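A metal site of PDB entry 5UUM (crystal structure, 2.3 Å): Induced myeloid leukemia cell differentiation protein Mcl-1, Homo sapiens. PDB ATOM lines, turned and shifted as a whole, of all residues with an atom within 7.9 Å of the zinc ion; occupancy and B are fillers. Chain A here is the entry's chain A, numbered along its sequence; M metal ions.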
ATOM      1  N   LYS A  39       2.722  10.183 -13.261  1.00  0.00           N
ATOM      2  CA  LYS A  39       1.519  10.941 -13.577  1.00  0.00           C
ATOM      3  C   LYS A  39       1.455  11.310 -15.052  1.00  0.00           C
ATOM      4  O   LYS A  39       0.356  11.382 -15.624  1.00  0.00           O
ATOM      5  CB  LYS A  39       1.457  12.192 -12.696  1.00  0.00           C
ATOM      6  CG  LYS A  39       1.394  11.886 -11.199  1.00  0.00           C
ATOM      7  CD  LYS A  39       1.536  13.129 -10.345  1.00  0.00           C
ATOM      8  CE  LYS A  39       0.306  14.006 -10.402  1.00  0.00           C
ATOM      9  NZ  LYS A  39       0.413  15.168  -9.480  1.00  0.00           N
ATOM     10  N   ASP A 144       5.738  18.122 -15.993  1.00  0.00           N
ATOM     11  CA  ASP A 144       4.832  18.679 -14.992  1.00  0.00           C
ATOM     12  C   ASP A 144       3.803  19.597 -15.645  1.00  0.00           C
ATOM     13  O   ASP A 144       2.624  19.597 -15.271  1.00  0.00           O
ATOM     14  CB  ASP A 144       5.611  19.421 -13.911  1.00  0.00           C
ATOM     15  CG  ASP A 144       6.465  18.489 -13.060  1.00  0.00           C
ATOM     16  OD1 ASP A 144       5.964  17.428 -12.639  1.00  0.00           O
ATOM     17  OD2 ASP A 144       7.652  18.829 -12.819  1.00  0.00           O
ATOM     18  N   VAL A 147       1.316  17.329 -17.550  1.00  0.00           N
ATOM     19  CA  VAL A 147       0.332  16.746 -16.638  1.00  0.00           C
ATOM     20  C   VAL A 147      -0.749  17.771 -16.317  1.00  0.00           C
ATOM     21  O   VAL A 147      -1.952  17.481 -16.418  1.00  0.00           O
ATOM     22  CB  VAL A 147       1.028  16.230 -15.363  1.00  0.00           C
ATOM     23  CG1 VAL A 147       0.010  15.931 -14.267  1.00  0.00           C
ATOM     24  CG2 VAL A 147       1.839  14.986 -15.680  1.00  0.00           C
ATOM     25  N   GLU A 148      -0.340  18.973 -15.901  1.00  0.00           N
ATOM     26  CA  GLU A 148      -1.302  19.959 -15.411  1.00  0.00           C
ATOM     27  C   GLU A 148      -2.208  20.460 -16.527  1.00  0.00           C
ATOM     28  O   GLU A 148      -3.414  20.626 -16.333  1.00  0.00           O
ATOM     29  CB  GLU A 148      -0.560  21.123 -14.748  1.00  0.00           C
ATOM     30  CG  GLU A 148       0.134  20.740 -13.447  1.00  0.00           C
ATOM     31  CD  GLU A 148      -0.833  20.178 -12.421  1.00  0.00           C
ATOM     32  OE1 GLU A 148      -1.957  20.716 -12.309  1.00  0.00           O
ATOM     33  OE2 GLU A 148      -0.477  19.187 -11.739  1.00  0.00           O
ATOM     34  N   PHE A 149      -1.649  20.696 -17.721  1.00  0.00           N
ATOM     35  CA  PHE A 149      -2.463  21.186 -18.827  1.00  0.00           C
ATOM     36  C   PHE A 149      -3.672  20.288 -19.061  1.00  0.00           C
ATOM     37  O   PHE A 149      -4.788  20.776 -19.290  1.00  0.00           O
ATOM     38  CB  PHE A 149      -1.611  21.273 -20.095  1.00  0.00           C
ATOM     39  CG  PHE A 149      -2.391  21.642 -21.319  1.00  0.00           C
ATOM     40  CD1 PHE A 149      -2.593  22.971 -21.652  1.00  0.00           C
ATOM     41  CD2 PHE A 149      -2.920  20.664 -22.148  1.00  0.00           C
ATOM     42  CE1 PHE A 149      -3.314  23.315 -22.773  1.00  0.00           C
ATOM     43  CE2 PHE A 149      -3.636  21.001 -23.273  1.00  0.00           C
ATOM     44  CZ  PHE A 149      -3.827  22.326 -23.590  1.00  0.00           C
ATOM     45  N   PHE A 150      -3.474  18.969 -19.002  1.00  0.00           N
ATOM     46  CA  PHE A 150      -4.533  18.005 -19.250  1.00  0.00           C
ATOM     47  C   PHE A 150      -5.232  17.548 -17.969  1.00  0.00           C
ATOM     48  O   PHE A 150      -6.022  16.601 -18.015  1.00  0.00           O
ATOM     49  CB  PHE A 150      -3.977  16.787 -19.989  1.00  0.00           C
ATOM     50  CG  PHE A 150      -3.557  17.077 -21.397  1.00  0.00           C
ATOM     51  CD1 PHE A 150      -4.501  17.388 -22.365  1.00  0.00           C
ATOM     52  CD2 PHE A 150      -2.215  17.036 -21.765  1.00  0.00           C
ATOM     53  CE1 PHE A 150      -4.122  17.650 -23.667  1.00  0.00           C
ATOM     54  CE2 PHE A 150      -1.836  17.297 -23.066  1.00  0.00           C
ATOM     55  CZ  PHE A 150      -2.786  17.608 -24.019  1.00  0.00           C
ATOM     56  N   HIS A 151      -4.957  18.179 -16.833  1.00  0.00           N
ATOM     57  CA  HIS A 151      -5.559  17.797 -15.564  1.00  0.00           C
ATOM     58  C   HIS A 151      -6.801  18.635 -15.319  1.00  0.00           C
ATOM     59  O   HIS A 151      -6.724  19.866 -15.199  1.00  0.00           O
ATOM     60  CB  HIS A 151      -4.567  17.969 -14.416  1.00  0.00           C
ATOM     61  CG  HIS A 151      -5.096  17.529 -13.086  1.00  0.00           C
ATOM     62  ND1 HIS A 151      -4.849  18.218 -11.920  1.00  0.00           N
ATOM     63  CD2 HIS A 151      -5.884  16.482 -12.740  1.00  0.00           C
ATOM     64  CE1 HIS A 151      -5.437  17.612 -10.909  1.00  0.00           C
ATOM     65  NE2 HIS A 151      -6.078  16.551 -11.389  1.00  0.00           N
ATOM     66  N   VAL A 152      -7.955  17.974 -15.218  1.00  0.00           N
ATOM     67  CA  VAL A 152      -9.213  18.643 -14.920  1.00  0.00           C
ATOM     68  C   VAL A 152      -9.279  18.889 -13.427  1.00  0.00           C
ATOM     69  O   VAL A 152      -9.228  17.944 -12.632  1.00  0.00           O
ATOM     70  CB  VAL A 152     -10.407  17.821 -15.405  1.00  0.00           C
ATOM     71  CG1 VAL A 152     -11.697  18.620 -15.280  1.00  0.00           C
ATOM     72  CG2 VAL A 152     -10.194  17.365 -16.841  1.00  0.00           C
ATOM     73  N   GLU A 153      -9.408  20.158 -13.032  1.00  0.00           N
ATOM     74  CA  GLU A 153      -9.275  20.534 -11.632  1.00  0.00           C
ATOM     75  C   GLU A 153     -10.601  20.545 -10.880  1.00  0.00           C
ATOM     76  O   GLU A 153     -10.599  20.390  -9.652  1.00  0.00           O
ATOM     77  CB  GLU A 153      -8.610  21.903 -11.521  1.00  0.00           C
ATOM     78  CG  GLU A 153      -7.165  21.919 -11.995  1.00  0.00           C
ATOM     79  CD  GLU A 153      -6.247  21.150 -11.071  1.00  0.00           C
ATOM     80  OE1 GLU A 153      -6.735  20.651 -10.032  1.00  0.00           O
ATOM     81  OE2 GLU A 153      -5.041  21.053 -11.372  1.00  0.00           O
HETATM   82 ZN    ZN M   1      -3.740  19.844 -11.363  1.00  0.00          ZN
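OE2 of Glu 153 binds the zinc ion, 1.8 Å away.
A ring nitrogen (ND1) of His 151 binds the zinc ion.
The side-chain carboxylate (OE1) of Glu 148 binds the zinc ion, 2.2 Å away.
Three residues have an atom within 4 Å of the zinc ion: Glu 148, His 151 and Glu 153.
Along chain A the residues within 4 Å of the zinc ion span positions 148 to 153.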
